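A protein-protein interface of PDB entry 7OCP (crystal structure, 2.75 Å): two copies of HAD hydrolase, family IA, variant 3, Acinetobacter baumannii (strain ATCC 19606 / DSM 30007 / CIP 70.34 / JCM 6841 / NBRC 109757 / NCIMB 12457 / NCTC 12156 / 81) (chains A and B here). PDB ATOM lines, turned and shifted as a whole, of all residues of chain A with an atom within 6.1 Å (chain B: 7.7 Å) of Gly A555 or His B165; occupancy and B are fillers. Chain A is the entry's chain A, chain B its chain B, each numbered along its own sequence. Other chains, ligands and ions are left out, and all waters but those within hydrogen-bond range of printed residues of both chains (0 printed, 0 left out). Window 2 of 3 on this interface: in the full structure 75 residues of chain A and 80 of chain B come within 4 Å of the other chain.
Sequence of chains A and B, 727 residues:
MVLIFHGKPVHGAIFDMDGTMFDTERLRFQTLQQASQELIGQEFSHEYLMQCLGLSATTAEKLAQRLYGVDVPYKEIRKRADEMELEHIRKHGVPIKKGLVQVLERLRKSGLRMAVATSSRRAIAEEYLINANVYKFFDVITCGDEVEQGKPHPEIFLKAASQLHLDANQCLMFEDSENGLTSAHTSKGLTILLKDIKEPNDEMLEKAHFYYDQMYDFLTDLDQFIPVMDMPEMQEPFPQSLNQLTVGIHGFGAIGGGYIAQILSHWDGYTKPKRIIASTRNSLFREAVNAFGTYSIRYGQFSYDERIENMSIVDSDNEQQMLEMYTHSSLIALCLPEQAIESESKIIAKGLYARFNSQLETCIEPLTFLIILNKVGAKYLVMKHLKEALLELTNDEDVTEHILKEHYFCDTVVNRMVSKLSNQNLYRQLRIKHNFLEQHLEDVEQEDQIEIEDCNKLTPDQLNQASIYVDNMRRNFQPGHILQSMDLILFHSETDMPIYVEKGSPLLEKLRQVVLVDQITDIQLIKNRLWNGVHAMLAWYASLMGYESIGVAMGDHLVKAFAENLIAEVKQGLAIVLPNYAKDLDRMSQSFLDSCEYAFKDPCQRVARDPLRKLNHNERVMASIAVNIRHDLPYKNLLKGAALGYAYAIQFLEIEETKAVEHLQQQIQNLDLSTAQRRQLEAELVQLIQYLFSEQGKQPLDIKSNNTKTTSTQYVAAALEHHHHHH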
ATOM      1  N   ILE A 550      -6.782   1.715   8.938  1.00  0.00           N
ATOM      2  CA  ILE A 550      -5.929   2.889   8.583  1.00  0.00           C
ATOM      3  C   ILE A 550      -4.581   2.377   8.054  1.00  0.00           C
ATOM      4  O   ILE A 550      -3.941   3.108   7.276  1.00  0.00           O
ATOM      5  CB  ILE A 550      -5.773   3.836   9.791  1.00  0.00           C
ATOM      6  CG1 ILE A 550      -5.400   5.258   9.363  1.00  0.00           C
ATOM      7  CG2 ILE A 550      -4.789   3.277  10.811  1.00  0.00           C
ATOM      8  CD1 ILE A 550      -5.718   6.307  10.402  1.00  0.00           C
ATOM      9  N   GLY A 551      -4.176   1.170   8.469  1.00  0.00           N
ATOM     10  CA  GLY A 551      -2.964   0.473   7.993  1.00  0.00           C
ATOM     11  C   GLY A 551      -3.085   0.045   6.539  1.00  0.00           C
ATOM     12  O   GLY A 551      -2.106   0.231   5.791  1.00  0.00           O
ATOM     13  N   VAL A 552      -4.235  -0.521   6.155  1.00  0.00           N
ATOM     14  CA  VAL A 552      -4.559  -0.920   4.751  1.00  0.00           C
ATOM     15  C   VAL A 552      -4.509   0.331   3.865  1.00  0.00           C
ATOM     16  O   VAL A 552      -3.884   0.265   2.789  1.00  0.00           O
ATOM     17  CB  VAL A 552      -5.927  -1.627   4.658  1.00  0.00           C
ATOM     18  CG1 VAL A 552      -6.519  -1.570   3.256  1.00  0.00           C
ATOM     19  CG2 VAL A 552      -5.850  -3.067   5.140  1.00  0.00           C
ATOM     20  N   ALA A 553      -5.135   1.422   4.320  1.00  0.00           N
ATOM     21  CA  ALA A 553      -5.319   2.694   3.580  1.00  0.00           C
ATOM     22  C   ALA A 553      -3.969   3.253   3.105  1.00  0.00           C
ATOM     23  O   ALA A 553      -3.940   3.846   2.010  1.00  0.00           O
ATOM     24  CB  ALA A 553      -6.048   3.691   4.447  1.00  0.00           C
ATOM     25  N   MET A 554      -2.902   3.064   3.890  1.00  0.00           N
ATOM     26  CA  MET A 554      -1.536   3.588   3.600  1.00  0.00           C
ATOM     27  C   MET A 554      -0.964   2.929   2.335  1.00  0.00           C
ATOM     28  O   MET A 554       0.012   3.480   1.785  1.00  0.00           O
ATOM     29  CB  MET A 554      -0.587   3.342   4.778  1.00  0.00           C
ATOM     30  CG  MET A 554      -0.937   4.152   6.014  1.00  0.00           C
ATOM     31  SD  MET A 554      -0.560   5.915   5.842  1.00  0.00           S
ATOM     32  CE  MET A 554       1.208   5.903   6.133  1.00  0.00           C
ATOM     33  N   GLY A 555      -1.532   1.796   1.903  1.00  0.00           N
ATOM     34  CA  GLY A 555      -1.242   1.162   0.601  1.00  0.00           C
ATOM     35  C   GLY A 555      -1.533   2.104  -0.555  1.00  0.00           C
ATOM     36  O   GLY A 555      -0.698   2.181  -1.478  1.00  0.00           O
ATOM     37  N   ASP A 556      -2.679   2.793  -0.503  1.00  0.00           N
ATOM     38  CA  ASP A 556      -3.050   3.891  -1.436  1.00  0.00           C
ATOM     39  C   ASP A 556      -2.104   5.069  -1.178  1.00  0.00           C
ATOM     40  O   ASP A 556      -2.073   5.557  -0.032  1.00  0.00           O
ATOM     41  CB  ASP A 556      -4.520   4.285  -1.261  1.00  0.00           C
ATOM     42  CG  ASP A 556      -5.052   5.240  -2.318  1.00  0.00           C
ATOM     43  OD1 ASP A 556      -4.573   5.176  -3.467  1.00  0.00           O
ATOM     44  OD2 ASP A 556      -5.950   6.037  -1.983  1.00  0.00           O
ATOM     45  N   HIS A 557      -1.358   5.496  -2.202  1.00  0.00           N
ATOM     46  CA  HIS A 557      -0.279   6.517  -2.104  1.00  0.00           C
ATOM     47  C   HIS A 557      -0.871   7.910  -1.837  1.00  0.00           C
ATOM     48  O   HIS A 557      -0.113   8.783  -1.374  1.00  0.00           O
ATOM     49  CB  HIS A 557       0.613   6.483  -3.355  1.00  0.00           C
ATOM     50  CG  HIS A 557       1.511   5.291  -3.419  1.00  0.00           C
ATOM     51  ND1 HIS A 557       1.529   4.431  -4.502  1.00  0.00           N
ATOM     52  CD2 HIS A 557       2.416   4.808  -2.537  1.00  0.00           C
ATOM     53  CE1 HIS A 557       2.410   3.474  -4.287  1.00  0.00           C
ATOM     54  NE2 HIS A 557       2.967   3.682  -3.087  1.00  0.00           N
ATOM     55  N   VAL A 559      -3.272   8.442   0.450  1.00  0.00           N
ATOM     56  CA  VAL A 559      -3.465   8.427   1.933  1.00  0.00           C
ATOM     57  C   VAL A 559      -2.121   8.721   2.610  1.00  0.00           C
ATOM     58  O   VAL A 559      -2.086   9.602   3.492  1.00  0.00           O
ATOM     59  CB  VAL A 559      -4.049   7.086   2.422  1.00  0.00           C
ATOM     60  CG1 VAL A 559      -4.200   7.053   3.936  1.00  0.00           C
ATOM     61  CG2 VAL A 559      -5.377   6.758   1.752  1.00  0.00           C
ATOM     62  N   LYS A 560      -1.066   8.001   2.215  1.00  0.00           N
ATOM     63  CA  LYS A 560       0.301   8.104   2.797  1.00  0.00           C
ATOM     64  C   LYS A 560       0.858   9.512   2.555  1.00  0.00           C
ATOM     65  O   LYS A 560       1.450  10.077   3.493  1.00  0.00           O
ATOM     66  CB  LYS A 560       1.217   7.029   2.203  1.00  0.00           C
ATOM     67  CG  LYS A 560       2.589   6.917   2.854  1.00  0.00           C
ATOM     68  CD  LYS A 560       3.295   5.610   2.559  1.00  0.00           C
ATOM     69  CE  LYS A 560       4.645   5.506   3.234  1.00  0.00           C
ATOM     70  NZ  LYS A 560       5.272   4.180   3.012  1.00  0.00           N
ATOM     71  N   CYS A 596       1.401   4.143  11.942  1.00  0.00           N
ATOM     72  CA  CYS A 596       0.289   4.244  10.955  1.00  0.00           C
ATOM     73  C   CYS A 596       0.465   3.230   9.817  1.00  0.00           C
ATOM     74  O   CYS A 596      -0.564   2.775   9.280  1.00  0.00           O
ATOM     75  CB  CYS A 596       0.202   5.643  10.356  1.00  0.00           C
ATOM     76  SG  CYS A 596      -0.554   6.854  11.471  1.00  0.00           S
ATOM     77  N   GLU A 597       1.714   2.906   9.462  1.00  0.00           N
ATOM     78  CA  GLU A 597       2.069   2.057   8.292  1.00  0.00           C
ATOM     79  C   GLU A 597       1.274   0.747   8.349  1.00  0.00           C
ATOM     80  O   GLU A 597       0.375   0.579   7.505  1.00  0.00           O
ATOM     81  CB  GLU A 597       3.579   1.810   8.238  1.00  0.00           C
ATOM     82  CG  GLU A 597       4.070   1.378   6.866  1.00  0.00           C
ATOM     83  CD  GLU A 597       3.962   2.441   5.784  1.00  0.00           C
ATOM     84  OE1 GLU A 597       3.635   2.081   4.636  1.00  0.00           O
ATOM     85  OE2 GLU A 597       4.209   3.625   6.091  1.00  0.00           O
ATOM     86  N   TYR A 598       1.573  -0.130   9.314  1.00  0.00           N
ATOM     87  CA  TYR A 598       0.934  -1.462   9.480  1.00  0.00           C
ATOM     88  C   TYR A 598       0.036  -1.445  10.724  1.00  0.00           C
ATOM     89  O   TYR A 598       0.247  -2.268  11.638  1.00  0.00           O
ATOM     90  CB  TYR A 598       1.998  -2.563   9.538  1.00  0.00           C
ATOM     91  CG  TYR A 598       2.871  -2.651   8.311  1.00  0.00           C
ATOM     92  CD1 TYR A 598       2.315  -2.799   7.048  1.00  0.00           C
ATOM     93  CD2 TYR A 598       4.253  -2.592   8.405  1.00  0.00           C
ATOM     94  CE1 TYR A 598       3.105  -2.878   5.913  1.00  0.00           C
ATOM     95  CE2 TYR A 598       5.058  -2.673   7.280  1.00  0.00           C
ATOM     96  CZ  TYR A 598       4.483  -2.815   6.029  1.00  0.00           C
ATOM     97  OH  TYR A 598       5.267  -2.895   4.916  1.00  0.00           O
ATOM     98  N   PHE A 600      -3.177  -2.426  11.186  1.00  0.00           N
ATOM     99  CA  PHE A 600      -4.276  -3.299  10.696  1.00  0.00           C
ATOM    100  C   PHE A 600      -5.287  -3.554  11.821  1.00  0.00           C
ATOM    101  O   PHE A 600      -6.501  -3.575  11.538  1.00  0.00           O
ATOM    102  CB  PHE A 600      -3.720  -4.622  10.160  1.00  0.00           C
ATOM    103  CG  PHE A 600      -2.767  -4.488   8.999  1.00  0.00           C
ATOM    104  CD1 PHE A 600      -3.212  -4.038   7.765  1.00  0.00           C
ATOM    105  CD2 PHE A 600      -1.427  -4.822   9.134  1.00  0.00           C
ATOM    106  CE1 PHE A 600      -2.338  -3.918   6.696  1.00  0.00           C
ATOM    107  CE2 PHE A 600      -0.554  -4.702   8.063  1.00  0.00           C
ATOM    108  CZ  PHE A 600      -1.011  -4.250   6.845  1.00  0.00           C
ATOM    109  N   HIS B  11      13.280  -3.192  -1.930  1.00  0.00           N
ATOM    110  CA  HIS B  11      12.539  -2.560  -0.802  1.00  0.00           C
ATOM    111  C   HIS B  11      11.761  -3.609   0.009  1.00  0.00           C
ATOM    112  O   HIS B  11      11.445  -3.314   1.178  1.00  0.00           O
ATOM    113  CB  HIS B  11      11.617  -1.451  -1.326  1.00  0.00           C
ATOM    114  CG  HIS B  11      12.349  -0.279  -1.889  1.00  0.00           C
ATOM    115  ND1 HIS B  11      12.838  -0.263  -3.181  1.00  0.00           N
ATOM    116  CD2 HIS B  11      12.675   0.914  -1.346  1.00  0.00           C
ATOM    117  CE1 HIS B  11      13.435   0.889  -3.408  1.00  0.00           C
ATOM    118  NE2 HIS B  11      13.349   1.629  -2.298  1.00  0.00           N
ATOM    119  N   ARG B 113      10.646  -4.711   3.782  1.00  0.00           N
ATOM    120  CA  ARG B 113       9.240  -4.979   4.184  1.00  0.00           C
ATOM    121  C   ARG B 113       8.847  -6.346   3.609  1.00  0.00           C
ATOM    122  O   ARG B 113       8.596  -6.427   2.392  1.00  0.00           O
ATOM    123  CB  ARG B 113       8.331  -3.835   3.720  1.00  0.00           C
ATOM    124  CG  ARG B 113       9.020  -2.477   3.665  1.00  0.00           C
ATOM    125  CD  ARG B 113       8.105  -1.307   3.977  1.00  0.00           C
ATOM    126  NE  ARG B 113       8.060  -1.017   5.407  1.00  0.00           N
ATOM    127  CZ  ARG B 113       7.574   0.099   5.949  1.00  0.00           C
ATOM    128  NH1 ARG B 113       7.589   0.252   7.264  1.00  0.00           N
ATOM    129  NH2 ARG B 113       7.076   1.060   5.185  1.00  0.00           N
ATOM    130  N   VAL B 140       2.981  -8.963   6.776  1.00  0.00           N
ATOM    131  CA  VAL B 140       1.681  -9.547   6.321  1.00  0.00           C
ATOM    132  C   VAL B 140       1.962 -10.898   5.650  1.00  0.00           C
ATOM    133  O   VAL B 140       3.116 -11.120   5.244  1.00  0.00           O
ATOM    134  CB  VAL B 140       0.940  -8.583   5.373  1.00  0.00           C
ATOM    135  CG1 VAL B 140       1.667  -8.413   4.046  1.00  0.00           C
ATOM    136  CG2 VAL B 140      -0.504  -9.005   5.143  1.00  0.00           C
ATOM    137  N   LYS B 159      -1.198  -9.117  -4.496  1.00  0.00           N
ATOM    138  CA  LYS B 159      -1.924  -8.814  -3.231  1.00  0.00           C
ATOM    139  C   LYS B 159      -0.929  -8.752  -2.065  1.00  0.00           C
ATOM    140  O   LYS B 159      -1.150  -7.934  -1.150  1.00  0.00           O
ATOM    141  CB  LYS B 159      -3.010  -9.865  -2.973  1.00  0.00           C
ATOM    142  CG  LYS B 159      -3.940  -9.565  -1.805  1.00  0.00           C
ATOM    143  CD  LYS B 159      -5.095 -10.539  -1.689  1.00  0.00           C
ATOM    144  CE  LYS B 159      -6.041 -10.211  -0.553  1.00  0.00           C
ATOM    145  NZ  LYS B 159      -5.357 -10.240   0.762  1.00  0.00           N
ATOM    146  N   ALA B 160       0.113  -9.589  -2.094  1.00  0.00           N
ATOM    147  CA  ALA B 160       1.199  -9.634  -1.085  1.00  0.00           C
ATOM    148  C   ALA B 160       1.986  -8.318  -1.118  1.00  0.00           C
ATOM    149  O   ALA B 160       2.184  -7.723  -0.042  1.00  0.00           O
ATOM    150  CB  ALA B 160       2.097 -10.819  -1.339  1.00  0.00           C
ATOM    151  N   ALA B 161       2.405  -7.886  -2.311  1.00  0.00           N
ATOM    152  CA  ALA B 161       3.189  -6.649  -2.551  1.00  0.00           C
ATOM    153  C   ALA B 161       2.343  -5.415  -2.214  1.00  0.00           C
ATOM    154  O   ALA B 161       2.907  -4.445  -1.675  1.00  0.00           O
ATOM    155  CB  ALA B 161       3.671  -6.610  -3.981  1.00  0.00           C
ATOM    156  N   SER B 162       1.042  -5.456  -2.530  1.00  0.00           N
ATOM    157  CA  SER B 162       0.065  -4.358  -2.297  1.00  0.00           C
ATOM    158  C   SER B 162      -0.093  -4.095  -0.793  1.00  0.00           C
ATOM    159  O   SER B 162      -0.154  -2.911  -0.409  1.00  0.00           O
ATOM    160  CB  SER B 162      -1.262  -4.670  -2.941  1.00  0.00           C
ATOM    161  OG  SER B 162      -2.151  -3.569  -2.833  1.00  0.00           O
ATOM    162  N   GLN B 163      -0.152  -5.156   0.019  1.00  0.00           N
ATOM    163  CA  GLN B 163      -0.358  -5.083   1.492  1.00  0.00           C
ATOM    164  C   GLN B 163       0.931  -4.628   2.189  1.00  0.00           C
ATOM    165  O   GLN B 163       0.834  -4.142   3.333  1.00  0.00           O
ATOM    166  CB  GLN B 163      -0.836  -6.433   2.031  1.00  0.00           C
ATOM    167  CG  GLN B 163      -2.288  -6.737   1.689  1.00  0.00           C
ATOM    168  CD  GLN B 163      -2.712  -8.126   2.103  1.00  0.00           C
ATOM    169  OE1 GLN B 163      -3.731  -8.313   2.762  1.00  0.00           O
ATOM    170  NE2 GLN B 163      -1.928  -9.118   1.714  1.00  0.00           N
ATOM    171  N   LEU B 164       2.089  -4.785   1.533  1.00  0.00           N
ATOM    172  CA  LEU B 164       3.402  -4.260   2.003  1.00  0.00           C
ATOM    173  C   LEU B 164       3.528  -2.774   1.640  1.00  0.00           C
ATOM    174  O   LEU B 164       4.468  -2.129   2.143  1.00  0.00           O
ATOM    175  CB  LEU B 164       4.537  -5.068   1.364  1.00  0.00           C
ATOM    176  CG  LEU B 164       4.703  -6.500   1.871  1.00  0.00           C
ATOM    177  CD1 LEU B 164       5.668  -7.273   0.983  1.00  0.00           C
ATOM    178  CD2 LEU B 164       5.173  -6.514   3.318  1.00  0.00           C
ATOM    179  N   HIS B 165       2.625  -2.266   0.794  1.00  0.00           N
ATOM    180  CA  HIS B 165       2.568  -0.856   0.316  1.00  0.00           C
ATOM    181  C   HIS B 165       3.774  -0.584  -0.594  1.00  0.00           C
ATOM    182  O   HIS B 165       4.391   0.493  -0.464  1.00  0.00           O
ATOM    183  CB  HIS B 165       2.460   0.114   1.503  1.00  0.00           C
ATOM    184  CG  HIS B 165       1.485  -0.323   2.544  1.00  0.00           C
ATOM    185  ND1 HIS B 165       1.719  -0.153   3.894  1.00  0.00           N
ATOM    186  CD2 HIS B 165       0.292  -0.950   2.443  1.00  0.00           C
ATOM    187  CE1 HIS B 165       0.703  -0.640   4.577  1.00  0.00           C
ATOM    188  NE2 HIS B 165      -0.186  -1.134   3.711  1.00  0.00           N
ATOM    189  N   LEU B 166       4.080  -1.538  -1.482  1.00  0.00           N
ATOM    190  CA  LEU B 166       5.170  -1.463  -2.492  1.00  0.00           C
ATOM    191  C   LEU B 166       4.643  -1.959  -3.843  1.00  0.00           C
ATOM    192  O   LEU B 166       3.512  -2.487  -3.887  1.00  0.00           O
ATOM    193  CB  LEU B 166       6.349  -2.325  -2.028  1.00  0.00           C
ATOM    194  CG  LEU B 166       7.110  -1.822  -0.803  1.00  0.00           C
ATOM    195  CD1 LEU B 166       8.053  -2.895  -0.279  1.00  0.00           C
ATOM    196  CD2 LEU B 166       7.879  -0.547  -1.123  1.00  0.00           C
ATOM    197  N   ASP B 167       5.446  -1.790  -4.898  1.00  0.00           N
ATOM    198  CA  ASP B 167       5.231  -2.403  -6.235  1.00  0.00           C
ATOM    199  C   ASP B 167       6.030  -3.710  -6.291  1.00  0.00           C
ATOM    200  O   ASP B 167       7.065  -3.798  -5.598  1.00  0.00           O
ATOM    201  CB  ASP B 167       5.626  -1.437  -7.356  1.00  0.00           C
ATOM    202  CG  ASP B 167       4.914  -0.095  -7.299  1.00  0.00           C
ATOM    203  OD1 ASP B 167       3.832  -0.027  -6.680  1.00  0.00           O
ATOM    204  OD2 ASP B 167       5.452   0.875  -7.871  1.00  0.00           O
ATOM    205  N   GLN B 170       9.827  -3.814  -6.951  1.00  0.00           N
ATOM    206  CA  GLN B 170      10.684  -3.383  -5.811  1.00  0.00           C
ATOM    207  C   GLN B 170      10.981  -4.571  -4.884  1.00  0.00           C
ATOM    208  O   GLN B 170      11.870  -4.424  -4.021  1.00  0.00           O
ATOM    209  CB  GLN B 170      10.003  -2.267  -5.013  1.00  0.00           C
ATOM    210  CG  GLN B 170       9.793  -0.982  -5.801  1.00  0.00           C
ATOM    211  CD  GLN B 170       9.056   0.062  -4.996  1.00  0.00           C
ATOM    212  OE1 GLN B 170       7.921  -0.141  -4.570  1.00  0.00           O
ATOM    213  NE2 GLN B 170       9.700   1.199  -4.788  1.00  0.00           N
ATOM    214  N   CYS B 171      10.273  -5.695  -5.052  1.00  0.00           N
ATOM    215  CA  CYS B 171      10.281  -6.859  -4.123  1.00  0.00           C
ATOM    216  C   CYS B 171      10.995  -8.061  -4.753  1.00  0.00           C
ATOM    217  O   CYS B 171      10.782  -8.313  -5.957  1.00  0.00           O
ATOM    218  CB  CYS B 171       8.861  -7.269  -3.750  1.00  0.00           C
ATOM    219  SG  CYS B 171       7.808  -5.876  -3.265  1.00  0.00           S
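The backbone carbonyl oxygen (O) of Gly A551 is in hydrogen-bond range of a ring nitrogen (NE2) of His B165, at 3.1 Å.
The side-chain carboxylate (OE1) of Glu A597 is in salt-bridge range of the guanidinium group (NH2) of Arg B113 (3.6 Å).
The side-chain carboxylate (OE1) of Glu A597 lies within hydrogen-bond range of a ring nitrogen (ND1) of His B165, 3.0 Å away.
The side-chain hydroxyl (OH) of Tyr A598 sits close to the guanidinium group (NE) of Arg B113, 3.4 Å away.
OH of Tyr A598 sits at hydrogen-bond distance from O of Leu B164 (3.0 Å).
No position is printed for both chains.
The side-chain amino group (NZ) of Lys A560 lies within salt-bridge range of the side-chain carboxylate (OE1) of Glu A597, 3.1 Å away.
The backbone carbonyl oxygen (O) of His B11 lies within hydrogen-bond range of the backbone NH (N) of Arg B113 (3.1 Å).
The backbone carbonyl oxygen of Lys B159 lies within hydrogen-bond range of the side-chain amide nitrogen of Gln B163 (3.2 Å).
The backbone carbonyl oxygen (O) of Gln B163 lies within hydrogen-bond range of a ring nitrogen (NE2) of His B165, 3.2 Å away.
Of chain B, only His B165 comes within 4 Å of Gly A555.
Printed residues of chain A within 4 Å of Arg B113: Glu A597 (3.5 Å) and Tyr A598 (3.4 Å).
Of the printed residues of chain A, Leu B164 touches Tyr A598.
His B165 touches just these residues of chain A: Gly A551 (3.1 Å), Gly A555 (3.2 Å), Glu A597 (3.0 Å) and Tyr A598 (3.5 Å).
The nearest residue of chain B that does not touch Gly A555 is Ser B162 (4.3 Å).
The nearest printed residue of chain A that does not touch His B165 is Val A552 (4.1 Å).
Among the printed residues, pairs that only touch across the chains: Gly A555 with His B165 (3.2 Å), Tyr A598 with Gln B163 (3.7 Å), Tyr A598 with His B165 (3.5 Å) and Phe A600 with Gln B163 (3.97 Å).
Hydrophobic or aromatic side chains of chain B within 4 Å of the printed part of chain A: Leu B164 and His B165.
Hydrophobic or aromatic side chains of chain A within 4 Å of the printed part of chain B: Tyr A598 and Phe A600.
Among the printed residues, 9 pairs touch across the chains.
Among the printed residues, Asp or Glu carboxylates within 4 Å of a Lys or Arg side-chain nitrogen of the other chain: Glu A597 with Arg B113 (3.6 Å).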
